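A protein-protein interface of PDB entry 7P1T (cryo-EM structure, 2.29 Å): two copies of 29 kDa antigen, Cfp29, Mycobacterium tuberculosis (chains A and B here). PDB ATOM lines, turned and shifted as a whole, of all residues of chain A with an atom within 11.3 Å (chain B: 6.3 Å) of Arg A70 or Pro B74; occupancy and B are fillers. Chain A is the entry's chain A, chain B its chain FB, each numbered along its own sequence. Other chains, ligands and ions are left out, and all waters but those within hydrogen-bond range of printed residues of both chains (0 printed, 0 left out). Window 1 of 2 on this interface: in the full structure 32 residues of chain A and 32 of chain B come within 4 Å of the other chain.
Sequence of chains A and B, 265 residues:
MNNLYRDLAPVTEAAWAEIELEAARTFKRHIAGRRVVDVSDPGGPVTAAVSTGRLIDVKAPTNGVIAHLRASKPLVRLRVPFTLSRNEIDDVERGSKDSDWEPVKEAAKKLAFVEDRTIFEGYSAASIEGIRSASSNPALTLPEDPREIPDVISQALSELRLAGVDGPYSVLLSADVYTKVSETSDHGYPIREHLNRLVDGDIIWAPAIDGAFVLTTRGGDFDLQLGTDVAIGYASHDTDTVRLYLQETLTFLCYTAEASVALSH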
ATOM      1  N   ALA A  48      21.912 -21.511   1.634  1.00  0.00           N
ATOM      2  CA  ALA A  48      21.310 -22.059   0.427  1.00  0.00           C
ATOM      3  C   ALA A  48      20.117 -21.249  -0.058  1.00  0.00           C
ATOM      4  O   ALA A  48      19.788 -21.275  -1.245  1.00  0.00           O
ATOM      5  CB  ALA A  48      20.884 -23.506   0.669  1.00  0.00           C
ATOM      6  N   ALA A  49      19.451 -20.540   0.847  1.00  0.00           N
ATOM      7  CA  ALA A  49      18.247 -19.812   0.487  1.00  0.00           C
ATOM      8  C   ALA A  49      18.096 -18.601   1.386  1.00  0.00           C
ATOM      9  O   ALA A  49      18.647 -18.534   2.483  1.00  0.00           O
ATOM     10  CB  ALA A  49      16.998 -20.695   0.588  1.00  0.00           C
ATOM     11  N   VAL A  50      17.339 -17.632   0.891  1.00  0.00           N
ATOM     12  CA  VAL A  50      17.018 -16.425   1.636  1.00  0.00           C
ATOM     13  C   VAL A  50      15.524 -16.430   1.907  1.00  0.00           C
ATOM     14  O   VAL A  50      14.721 -16.602   0.985  1.00  0.00           O
ATOM     15  CB  VAL A  50      17.443 -15.158   0.876  1.00  0.00           C
ATOM     16  CG1 VAL A  50      17.144 -13.922   1.702  1.00  0.00           C
ATOM     17  CG2 VAL A  50      18.917 -15.221   0.547  1.00  0.00           C
ATOM     18  N   SER A  51      15.158 -16.269   3.173  1.00  0.00           N
ATOM     19  CA  SER A  51      13.756 -16.189   3.550  1.00  0.00           C
ATOM     20  C   SER A  51      13.143 -14.888   3.058  1.00  0.00           C
ATOM     21  O   SER A  51      13.717 -13.813   3.237  1.00  0.00           O
ATOM     22  CB  SER A  51      13.615 -16.288   5.065  1.00  0.00           C
ATOM     23  OG  SER A  51      12.284 -16.039   5.460  1.00  0.00           O
ATOM     24  N   THR A  52      11.973 -14.987   2.437  1.00  0.00           N
ATOM     25  CA  THR A  52      11.218 -13.805   2.049  1.00  0.00           C
ATOM     26  C   THR A  52      10.200 -13.391   3.096  1.00  0.00           C
ATOM     27  O   THR A  52       9.742 -12.245   3.075  1.00  0.00           O
ATOM     28  CB  THR A  52      10.488 -14.048   0.730  1.00  0.00           C
ATOM     29  OG1 THR A  52       9.511 -15.070   0.917  1.00  0.00           O
ATOM     30  CG2 THR A  52      11.466 -14.497  -0.333  1.00  0.00           C
ATOM     31  N   GLY A  53       9.886 -14.303   4.022  1.00  0.00           N
ATOM     32  CA  GLY A  53       8.937 -13.991   5.108  1.00  0.00           C
ATOM     33  C   GLY A  53       7.499 -14.177   4.666  1.00  0.00           C
ATOM     34  O   GLY A  53       6.597 -13.765   5.417  1.00  0.00           O
ATOM     35  N   ARG A  54       7.260 -14.668   3.451  1.00  0.00           N
ATOM     36  CA  ARG A  54       5.866 -14.921   2.996  1.00  0.00           C
ATOM     37  C   ARG A  54       5.438 -16.363   3.293  1.00  0.00           C
ATOM     38  O   ARG A  54       6.292 -17.150   3.730  1.00  0.00           O
ATOM     39  CB  ARG A  54       5.685 -14.545   1.525  1.00  0.00           C
ATOM     40  CG  ARG A  54       6.339 -13.229   1.133  1.00  0.00           C
ATOM     41  CD  ARG A  54       5.678 -12.047   1.808  1.00  0.00           C
ATOM     42  NE  ARG A  54       5.121 -11.123   0.832  1.00  0.00           N
ATOM     43  CZ  ARG A  54       4.760  -9.876   1.101  1.00  0.00           C
ATOM     44  NH1 ARG A  54       4.897  -9.394   2.324  1.00  0.00           N
ATOM     45  NH2 ARG A  54       4.265  -9.114   0.144  1.00  0.00           N
ATOM     46  N   LEU A  55       4.173 -16.700   3.047  1.00  0.00           N
ATOM     47  CA  LEU A  55       3.626 -18.047   3.366  1.00  0.00           C
ATOM     48  C   LEU A  55       2.863 -18.599   2.157  1.00  0.00           C
ATOM     49  O   LEU A  55       2.210 -17.799   1.459  1.00  0.00           O
ATOM     50  CB  LEU A  55       2.703 -17.931   4.582  1.00  0.00           C
ATOM     51  CG  LEU A  55       3.399 -17.965   5.942  1.00  0.00           C
ATOM     52  CD1 LEU A  55       2.383 -17.874   7.067  1.00  0.00           C
ATOM     53  CD2 LEU A  55       4.244 -19.222   6.088  1.00  0.00           C
ATOM     54  N   ILE A  56       2.937 -19.910   1.925  1.00  0.00           N
ATOM     55  CA  ILE A  56       2.259 -20.537   0.793  1.00  0.00           C
ATOM     56  C   ILE A  56       1.247 -21.565   1.266  1.00  0.00           C
ATOM     57  O   ILE A  56       1.610 -22.537   1.925  1.00  0.00           O
ATOM     58  CB  ILE A  56       3.247 -21.258  -0.150  1.00  0.00           C
ATOM     59  CG1 ILE A  56       4.511 -20.428  -0.382  1.00  0.00           C
ATOM     60  CG2 ILE A  56       2.583 -21.575  -1.482  1.00  0.00           C
ATOM     61  CD1 ILE A  56       5.719 -21.265  -0.738  1.00  0.00           C
ATOM     62  N   ASP A  57      -0.018 -21.373   0.914  1.00  0.00           N
ATOM     63  CA  ASP A  57      -1.070 -22.310   1.314  1.00  0.00           C
ATOM     64  C   ASP A  57      -0.870 -23.706   0.752  1.00  0.00           C
ATOM     65  O   ASP A  57      -0.749 -23.874  -0.465  1.00  0.00           O
ATOM     66  CB  ASP A  57      -2.436 -21.786   0.865  1.00  0.00           C
ATOM     67  CG  ASP A  57      -2.852 -20.533   1.601  1.00  0.00           C
ATOM     68  OD1 ASP A  57      -2.257 -19.465   1.351  1.00  0.00           O
ATOM     69  OD2 ASP A  57      -3.775 -20.619   2.439  1.00  0.00           O
ATOM     70  N   VAL A  58      -0.831 -24.710   1.625  1.00  0.00           N
ATOM     71  CA  VAL A  58      -0.729 -26.100   1.155  1.00  0.00           C
ATOM     72  C   VAL A  58      -1.918 -26.938   1.601  1.00  0.00           C
ATOM     73  O   VAL A  58      -2.578 -26.610   2.592  1.00  0.00           O
ATOM     74  CB  VAL A  58       0.566 -26.814   1.606  1.00  0.00           C
ATOM     75  CG1 VAL A  58       1.537 -26.905   0.445  1.00  0.00           C
ATOM     76  CG2 VAL A  58       1.199 -26.144   2.810  1.00  0.00           C
ATOM     77  N   ILE A  66      -4.025 -26.273   9.792  1.00  0.00           N
ATOM     78  CA  ILE A  66      -3.798 -25.288   8.768  1.00  0.00           C
ATOM     79  C   ILE A  66      -2.318 -25.253   8.533  1.00  0.00           C
ATOM     80  O   ILE A  66      -1.551 -24.986   9.445  1.00  0.00           O
ATOM     81  CB  ILE A  66      -4.328 -23.899   9.173  1.00  0.00           C
ATOM     82  CG1 ILE A  66      -5.843 -23.948   9.357  1.00  0.00           C
ATOM     83  CG2 ILE A  66      -3.961 -22.854   8.136  1.00  0.00           C
ATOM     84  CD1 ILE A  66      -6.407 -22.699   9.985  1.00  0.00           C
ATOM     85  N   ALA A  67      -1.913 -25.534   7.310  1.00  0.00           N
ATOM     86  CA  ALA A  67      -0.493 -25.601   6.997  1.00  0.00           C
ATOM     87  C   ALA A  67      -0.048 -24.575   6.002  1.00  0.00           C
ATOM     88  O   ALA A  67      -0.767 -24.249   5.070  1.00  0.00           O
ATOM     89  CB  ALA A  67      -0.159 -26.991   6.483  1.00  0.00           C
ATOM     90  N   HIS A  68       1.143 -24.060   6.210  1.00  0.00           N
ATOM     91  CA  HIS A  68       1.690 -23.122   5.269  1.00  0.00           C
ATOM     92  C   HIS A  68       3.165 -23.347   5.066  1.00  0.00           C
ATOM     93  O   HIS A  68       3.914 -23.480   6.018  1.00  0.00           O
ATOM     94  CB  HIS A  68       1.473 -21.687   5.760  1.00  0.00           C
ATOM     95  CG  HIS A  68       0.117 -21.138   5.478  1.00  0.00           C
ATOM     96  ND1 HIS A  68      -0.895 -21.146   6.410  1.00  0.00           N
ATOM     97  CD2 HIS A  68      -0.390 -20.541   4.375  1.00  0.00           C
ATOM     98  CE1 HIS A  68      -1.974 -20.595   5.889  1.00  0.00           C
ATOM     99  NE2 HIS A  68      -1.694 -20.217   4.656  1.00  0.00           N
ATOM    100  N   LEU A  69       3.598 -23.334   3.826  1.00  0.00           N
ATOM    101  CA  LEU A  69       5.012 -23.443   3.517  1.00  0.00           C
ATOM    102  C   LEU A  69       5.675 -22.078   3.598  1.00  0.00           C
ATOM    103  O   LEU A  69       5.120 -21.080   3.136  1.00  0.00           O
ATOM    104  CB  LEU A  69       5.215 -24.026   2.120  1.00  0.00           C
ATOM    105  CG  LEU A  69       4.905 -25.510   1.971  1.00  0.00           C
ATOM    106  CD1 LEU A  69       5.198 -25.952   0.560  1.00  0.00           C
ATOM    107  CD2 LEU A  69       5.712 -26.312   2.969  1.00  0.00           C
ATOM    108  N   ARG A  70       6.862 -22.038   4.189  1.00  0.00           N
ATOM    109  CA  ARG A  70       7.648 -20.814   4.164  1.00  0.00           C
ATOM    110  C   ARG A  70       8.236 -20.604   2.774  1.00  0.00           C
ATOM    111  O   ARG A  70       8.816 -21.524   2.187  1.00  0.00           O
ATOM    112  CB  ARG A  70       8.754 -20.867   5.211  1.00  0.00           C
ATOM    113  CG  ARG A  70       8.247 -20.865   6.639  1.00  0.00           C
ATOM    114  CD  ARG A  70       7.825 -19.479   7.098  1.00  0.00           C
ATOM    115  NE  ARG A  70       8.890 -18.502   6.925  1.00  0.00           N
ATOM    116  CZ  ARG A  70       9.537 -17.907   7.919  1.00  0.00           C
ATOM    117  NH1 ARG A  70       9.227 -18.182   9.175  1.00  0.00           N
ATOM    118  NH2 ARG A  70      10.496 -17.038   7.656  1.00  0.00           N
ATOM    119  N   ALA A  71       8.073 -19.399   2.241  1.00  0.00           N
ATOM    120  CA  ALA A  71       8.642 -19.051   0.951  1.00  0.00           C
ATOM    121  C   ALA A  71      10.099 -18.641   1.101  1.00  0.00           C
ATOM    122  O   ALA A  71      10.507 -18.089   2.124  1.00  0.00           O
ATOM    123  CB  ALA A  71       7.852 -17.914   0.302  1.00  0.00           C
ATOM    124  N   SER A  72      10.887 -18.915   0.067  1.00  0.00           N
ATOM    125  CA  SER A  72      12.295 -18.553   0.074  1.00  0.00           C
ATOM    126  C   SER A  72      12.780 -18.408  -1.358  1.00  0.00           C
ATOM    127  O   SER A  72      12.094 -18.775  -2.313  1.00  0.00           O
ATOM    128  CB  SER A  72      13.138 -19.583   0.837  1.00  0.00           C
ATOM    129  OG  SER A  72      13.090 -20.850   0.218  1.00  0.00           O
ATOM    130  N   LYS A  73      13.978 -17.852  -1.492  1.00  0.00           N
ATOM    131  CA  LYS A  73      14.650 -17.680  -2.770  1.00  0.00           C
ATOM    132  C   LYS A  73      15.934 -18.491  -2.772  1.00  0.00           C
ATOM    133  O   LYS A  73      16.761 -18.327  -1.860  1.00  0.00           O
ATOM    134  CB  LYS A  73      14.956 -16.208  -3.028  1.00  0.00           C
ATOM    135  CG  LYS A  73      13.741 -15.337  -3.184  1.00  0.00           C
ATOM    136  CD  LYS A  73      12.756 -15.916  -4.171  1.00  0.00           C
ATOM    137  CE  LYS A  73      11.950 -14.828  -4.825  1.00  0.00           C
ATOM    138  NZ  LYS A  73      11.102 -15.367  -5.913  1.00  0.00           N
ATOM    139  N   PRO A  74      16.145 -19.372  -3.741  1.00  0.00           N
ATOM    140  CA  PRO A  74      17.391 -20.144  -3.775  1.00  0.00           C
ATOM    141  C   PRO A  74      18.560 -19.321  -4.287  1.00  0.00           C
ATOM    142  O   PRO A  74      18.414 -18.472  -5.168  1.00  0.00           O
ATOM    143  CB  PRO A  74      17.061 -21.284  -4.743  1.00  0.00           C
ATOM    144  CG  PRO A  74      16.019 -20.707  -5.647  1.00  0.00           C
ATOM    145  CD  PRO A  74      15.216 -19.751  -4.820  1.00  0.00           C
ATOM    146  N   GLY B  44      14.312 -19.597  14.714  1.00  0.00           N
ATOM    147  CA  GLY B  44      13.747 -18.276  14.863  1.00  0.00           C
ATOM    148  C   GLY B  44      12.692 -18.048  13.808  1.00  0.00           C
ATOM    149  O   GLY B  44      12.521 -18.863  12.897  1.00  0.00           O
ATOM    150  N   PRO B  45      11.967 -16.932  13.916  1.00  0.00           N
ATOM    151  CA  PRO B  45      10.876 -16.668  12.966  1.00  0.00           C
ATOM    152  C   PRO B  45      11.340 -16.434  11.538  1.00  0.00           C
ATOM    153  O   PRO B  45      10.583 -16.712  10.604  1.00  0.00           O
ATOM    154  CB  PRO B  45      10.202 -15.420  13.554  1.00  0.00           C
ATOM    155  CG  PRO B  45      11.224 -14.808  14.426  1.00  0.00           C
ATOM    156  CD  PRO B  45      12.041 -15.911  14.973  1.00  0.00           C
ATOM    157  N   VAL B  46      12.566 -15.952  11.337  1.00  0.00           N
ATOM    158  CA  VAL B  46      12.999 -15.587   9.992  1.00  0.00           C
ATOM    159  C   VAL B  46      13.450 -16.817   9.217  1.00  0.00           C
ATOM    160  O   VAL B  46      13.580 -16.776   7.991  1.00  0.00           O
ATOM    161  CB  VAL B  46      14.110 -14.524  10.055  1.00  0.00           C
ATOM    162  CG1 VAL B  46      13.599 -13.276  10.718  1.00  0.00           C
ATOM    163  CG2 VAL B  46      15.318 -15.061  10.789  1.00  0.00           C
ATOM    164  N   THR B  47      13.700 -17.919   9.918  1.00  0.00           N
ATOM    165  CA  THR B  47      14.216 -19.128   9.290  1.00  0.00           C
ATOM    166  C   THR B  47      13.154 -19.755   8.399  1.00  0.00           C
ATOM    167  O   THR B  47      12.023 -19.982   8.832  1.00  0.00           O
ATOM    168  CB  THR B  47      14.663 -20.107  10.374  1.00  0.00           C
ATOM    169  OG1 THR B  47      15.672 -19.490  11.177  1.00  0.00           O
ATOM    170  CG2 THR B  47      15.236 -21.360   9.760  1.00  0.00           C
ATOM    171  N   ALA B  48      13.512 -20.020   7.147  1.00  0.00           N
ATOM    172  CA  ALA B  48      12.511 -20.432   6.172  1.00  0.00           C
ATOM    173  C   ALA B  48      12.852 -21.753   5.499  1.00  0.00           C
ATOM    174  O   ALA B  48      11.960 -22.459   5.025  1.00  0.00           O
ATOM    175  CB  ALA B  48      12.336 -19.345   5.114  1.00  0.00           C
ATOM    176  N   ALA B  49      14.135 -22.092   5.433  1.00  0.00           N
ATOM    177  CA  ALA B  49      14.556 -23.290   4.727  1.00  0.00           C
ATOM    178  C   ALA B  49      15.827 -23.830   5.352  1.00  0.00           C
ATOM    179  O   ALA B  49      16.574 -23.118   6.022  1.00  0.00           O
ATOM    180  CB  ALA B  49      14.782 -23.020   3.236  1.00  0.00           C
ATOM    181  N   VAL B  50      16.055 -25.117   5.127  1.00  0.00           N
ATOM    182  CA  VAL B  50      17.257 -25.795   5.582  1.00  0.00           C
ATOM    183  C   VAL B  50      18.049 -26.210   4.355  1.00  0.00           C
ATOM    184  O   VAL B  50      17.506 -26.845   3.445  1.00  0.00           O
ATOM    185  CB  VAL B  50      16.926 -27.005   6.470  1.00  0.00           C
ATOM    186  CG1 VAL B  50      18.200 -27.657   6.970  1.00  0.00           C
ATOM    187  CG2 VAL B  50      16.068 -26.573   7.637  1.00  0.00           C
ATOM    188  N   SER B  72      17.310 -26.947  -1.120  1.00  0.00           N
ATOM    189  CA  SER B  72      16.920 -26.699   0.258  1.00  0.00           C
ATOM    190  C   SER B  72      15.577 -27.358   0.523  1.00  0.00           C
ATOM    191  O   SER B  72      14.890 -27.815  -0.391  1.00  0.00           O
ATOM    192  CB  SER B  72      16.865 -25.197   0.567  1.00  0.00           C
ATOM    193  OG  SER B  72      15.885 -24.545  -0.212  1.00  0.00           O
ATOM    194  N   LYS B  73      15.220 -27.410   1.801  1.00  0.00           N
ATOM    195  CA  LYS B  73      13.947 -27.943   2.261  1.00  0.00           C
ATOM    196  C   LYS B  73      13.159 -26.834   2.938  1.00  0.00           C
ATOM    197  O   LYS B  73      13.681 -26.190   3.862  1.00  0.00           O
ATOM    198  CB  LYS B  73      14.163 -29.102   3.229  1.00  0.00           C
ATOM    199  CG  LYS B  73      14.814 -30.311   2.618  1.00  0.00           C
ATOM    200  CD  LYS B  73      14.133 -30.729   1.338  1.00  0.00           C
ATOM    201  CE  LYS B  73      14.288 -32.209   1.107  1.00  0.00           C
ATOM    202  NZ  LYS B  73      13.484 -32.659  -0.053  1.00  0.00           N
ATOM    203  N   PRO B  74      11.928 -26.563   2.521  1.00  0.00           N
ATOM    204  CA  PRO B  74      11.142 -25.517   3.179  1.00  0.00           C
ATOM    205  C   PRO B  74      10.574 -25.979   4.510  1.00  0.00           C
ATOM    206  O   PRO B  74      10.200 -27.140   4.682  1.00  0.00           O
ATOM    207  CB  PRO B  74      10.020 -25.246   2.173  1.00  0.00           C
ATOM    208  CG  PRO B  74       9.862 -26.543   1.443  1.00  0.00           C
ATOM    209  CD  PRO B  74      11.223 -27.164   1.375  1.00  0.00           C
ATOM    210  N   LEU B  75      10.512 -25.054   5.463  1.00  0.00           N
ATOM    211  CA  LEU B  75       9.743 -25.287   6.674  1.00  0.00           C
ATOM    212  C   LEU B  75       8.253 -25.206   6.376  1.00  0.00           C
ATOM    213  O   LEU B  75       7.819 -24.524   5.445  1.00  0.00           O
ATOM    214  CB  LEU B  75      10.089 -24.262   7.747  1.00  0.00           C
ATOM    215  CG  LEU B  75      11.505 -24.218   8.303  1.00  0.00           C
ATOM    216  CD1 LEU B  75      11.587 -23.210   9.423  1.00  0.00           C
ATOM    217  CD2 LEU B  75      11.895 -25.565   8.805  1.00  0.00           C
ATOM    218  N   VAL B  76       7.463 -25.905   7.178  1.00  0.00           N
ATOM    219  CA  VAL B  76       6.013 -25.802   7.134  1.00  0.00           C
ATOM    220  C   VAL B  76       5.550 -25.307   8.497  1.00  0.00           C
ATOM    221  O   VAL B  76       6.070 -25.735   9.533  1.00  0.00           O
ATOM    222  CB  VAL B  76       5.344 -27.136   6.730  1.00  0.00           C
ATOM    223  CG1 VAL B  76       5.750 -28.297   7.630  1.00  0.00           C
ATOM    224  CG2 VAL B  76       3.829 -27.002   6.660  1.00  0.00           C
ATOM    225  N   ARG B  77       4.637 -24.342   8.490  1.00  0.00           N
ATOM    226  CA  ARG B  77       4.008 -23.870   9.709  1.00  0.00           C
ATOM    227  C   ARG B  77       2.671 -24.576   9.878  1.00  0.00           C
ATOM    228  O   ARG B  77       1.823 -24.544   8.983  1.00  0.00           O
ATOM    229  CB  ARG B  77       3.811 -22.356   9.688  1.00  0.00           C
ATOM    230  CG  ARG B  77       3.188 -21.816  10.957  1.00  0.00           C
ATOM    231  CD  ARG B  77       2.787 -20.371  10.803  1.00  0.00           C
ATOM    232  NE  ARG B  77       1.544 -20.230  10.064  1.00  0.00           N
ATOM    233  CZ  ARG B  77       0.826 -19.117  10.029  1.00  0.00           C
ATOM    234  NH1 ARG B  77       1.235 -18.050  10.696  1.00  0.00           N
ATOM    235  NH2 ARG B  77      -0.295 -19.074   9.329  1.00  0.00           N
ATOM    236  N   ALA B 125       3.290 -32.735   0.402  1.00  0.00           N
ATOM    237  CA  ALA B 125       3.072 -31.346   0.016  1.00  0.00           C
ATOM    238  C   ALA B 125       4.138 -30.431   0.605  1.00  0.00           C
ATOM    239  O   ALA B 125       4.484 -29.413  -0.002  1.00  0.00           O
ATOM    240  CB  ALA B 125       1.682 -30.897   0.454  1.00  0.00           C
ATOM    241  N   ALA B 126       4.680 -30.783   1.764  1.00  0.00           N
ATOM    242  CA  ALA B 126       5.773 -30.045   2.371  1.00  0.00           C
ATOM    243  C   ALA B 126       7.138 -30.602   2.002  1.00  0.00           C
ATOM    244  O   ALA B 126       8.133 -30.204   2.618  1.00  0.00           O
ATOM    245  CB  ALA B 126       5.618 -30.031   3.893  1.00  0.00           C
ATOM    246  N   SER B 127       7.191 -31.512   1.019  1.00  0.00           N
ATOM    247  CA  SER B 127       8.413 -32.168   0.534  1.00  0.00           C
ATOM    248  C   SER B 127       9.160 -32.889   1.651  1.00  0.00           C
ATOM    249  O   SER B 127      10.387 -32.873   1.712  1.00  0.00           O
ATOM    250  CB  SER B 127       9.334 -31.181  -0.183  1.00  0.00           C
ATOM    251  OG  SER B 127       8.681 -30.604  -1.292  1.00  0.00           O
ATOM    252  N   ILE B 128       8.416 -33.522   2.547  1.00  0.00           N
ATOM    253  CA  ILE B 128       8.991 -34.279   3.650  1.00  0.00           C
ATOM    254  C   ILE B 128       8.730 -35.748   3.385  1.00  0.00           C
ATOM    255  O   ILE B 128       7.575 -36.170   3.258  1.00  0.00           O
ATOM    256  CB  ILE B 128       8.406 -33.856   5.004  1.00  0.00           C
ATOM    257  CG1 ILE B 128       8.871 -32.454   5.373  1.00  0.00           C
ATOM    258  CG2 ILE B 128       8.817 -34.842   6.087  1.00  0.00           C
ATOM    259  CD1 ILE B 128       8.055 -31.820   6.477  1.00  0.00           C
ATOM    260  N   THR B 249       6.524 -24.469  13.610  1.00  0.00           N
ATOM    261  CA  THR B 249       7.055 -24.539  12.255  1.00  0.00           C
ATOM    262  C   THR B 249       8.312 -25.401  12.220  1.00  0.00           C
ATOM    263  O   THR B 249       9.209 -25.253  13.056  1.00  0.00           O
ATOM    264  CB  THR B 249       7.275 -23.126  11.665  1.00  0.00           C
ATOM    265  OG1 THR B 249       7.709 -23.217  10.302  1.00  0.00           O
ATOM    266  CG2 THR B 249       8.220 -22.272  12.476  1.00  0.00           C
ATOM    267  N   LEU B 250       8.354 -26.327  11.263  1.00  0.00           N
ATOM    268  CA  LEU B 250       9.359 -27.384  11.275  1.00  0.00           C
ATOM    269  C   LEU B 250       9.547 -27.981   9.889  1.00  0.00           C
ATOM    270  O   LEU B 250       8.744 -27.780   8.979  1.00  0.00           O
ATOM    271  CB  LEU B 250       8.990 -28.491  12.282  1.00  0.00           C
ATOM    272  CG  LEU B 250       7.691 -29.313  12.184  1.00  0.00           C
ATOM    273  CD1 LEU B 250       7.721 -30.525  11.248  1.00  0.00           C
ATOM    274  CD2 LEU B 250       7.335 -29.781  13.570  1.00  0.00           C
ATOM    275  N   THR B 251      10.642 -28.730   9.756  1.00  0.00           N
ATOM    276  CA  THR B 251      10.807 -29.713   8.694  1.00  0.00           C
ATOM    277  C   THR B 251      11.507 -30.918   9.299  1.00  0.00           C
ATOM    278  O   THR B 251      12.045 -30.844  10.405  1.00  0.00           O
ATOM    279  CB  THR B 251      11.607 -29.183   7.491  1.00  0.00           C
ATOM    280  OG1 THR B 251      11.625 -30.178   6.465  1.00  0.00           O
ATOM    281  CG2 THR B 251      13.040 -28.907   7.885  1.00  0.00           C
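The backbone NH (N) of Arg A70 lies within hydrogen-bond range of the backbone carbonyl oxygen (O) of Leu B75. The backbone carbonyl oxygen of Thr B47 lies within hydrogen-bond range of the guanidinium group of Arg A70 (3.3 Å). The backbone carbonyl oxygen of Ile A66 lies close to the backbone carbonyl oxygen of Arg B77 (3.4 Å). O of His A68 sits at hydrogen-bond distance from N of Arg B77. The backbone carbonyl oxygen (O) of Val B46 lies within hydrogen-bond range of the side-chain hydroxyl (OG) of Ser A51 (2.9 Å). NH2 of Arg A70 is in hydrogen-bond range of O of Val B46 (3.1 Å). NH1 of Arg A70 lies within hydrogen-bond range of O of Pro B45 (2.5 Å).
6 positions are printed for both chains.
Of the 20 printed residues of chain B, 10 touch a printed residue of chain A. Of the 20 printed residues of chain A, 9 touch a printed residue of chain B. Among the printed residues, 20 pairs touch across the chains.
The backbone carbonyl oxygen of Leu A69 lies within hydrogen-bond range of the backbone NH of Ile A56 (2.8 Å). OG1 of Thr B249 lies within hydrogen-bond range of O of Val B76 (3.1 Å). The backbone NH (N) of Val B76 is in hydrogen-bond range of the backbone carbonyl oxygen (O) of Leu B250 (2.9 Å). The backbone NH (N) of Val A58 sits at hydrogen-bond distance from the backbone carbonyl oxygen (O) of Ala A67 (3.5 Å). The backbone NH (N) of Ala A71 lies within hydrogen-bond range of the backbone carbonyl oxygen (O) of Arg A54 (3.2 Å). OG1 of Thr A52 sits close to O of Ala A71.
Among the printed residues, merely in contact across the chains: Ala A67 with Arg B77, Ser A51 with Ala B48, His A68 with Val B76, Leu A55 with Arg B77, Leu A69 with Leu B75, Leu A69 with Ala B125, Arg A70 with Ala B48, Ala A71 with Ala B48, Leu A69 with Ala B126, Leu A69 with Val B76, Val A58 with Ala B125, Arg A70 with Pro B74 and Ala A67 with Val B76.
Arg A70 touches six residues of chain B. Printed residues of chain A within 4 Å of Pro B45: Arg A70 (2.5 Å). Thr B47 touches one residue of chain A. Of chain A, only Ser A51 (3.3 Å), Arg A70 (3.6 Å) and Ala A71 (3.7 Å) come within 4 Å of Ala B48. Of chain A, only Leu A69 (3.6 Å) and Arg A70 (2.9 Å) come within 4 Å of Leu B75. Ala B126 touches just one residue of chain A: Leu A69 (3.8 Å). No residue of chain A comes within 4 Å of Thr B251. Of the printed residues of chain A, Ala B125 touches Val A58 (3.9 Å) and Leu A69 (3.6 Å). Printed residues of chain B within 4 Å of Ala A67: Val B76 and Arg B77. Of the printed residues of chain B, Leu A55 touches Arg B77 (3.6 Å). Of the printed residues of chain B, Ala A71 touches Ala B48. Gly A53 touches none of the printed residues of chain B. Val A50 touches none of the printed residues of chain B. The nearest residue of chain A that does not touch Pro B74 is Leu A69 (4.4 Å).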
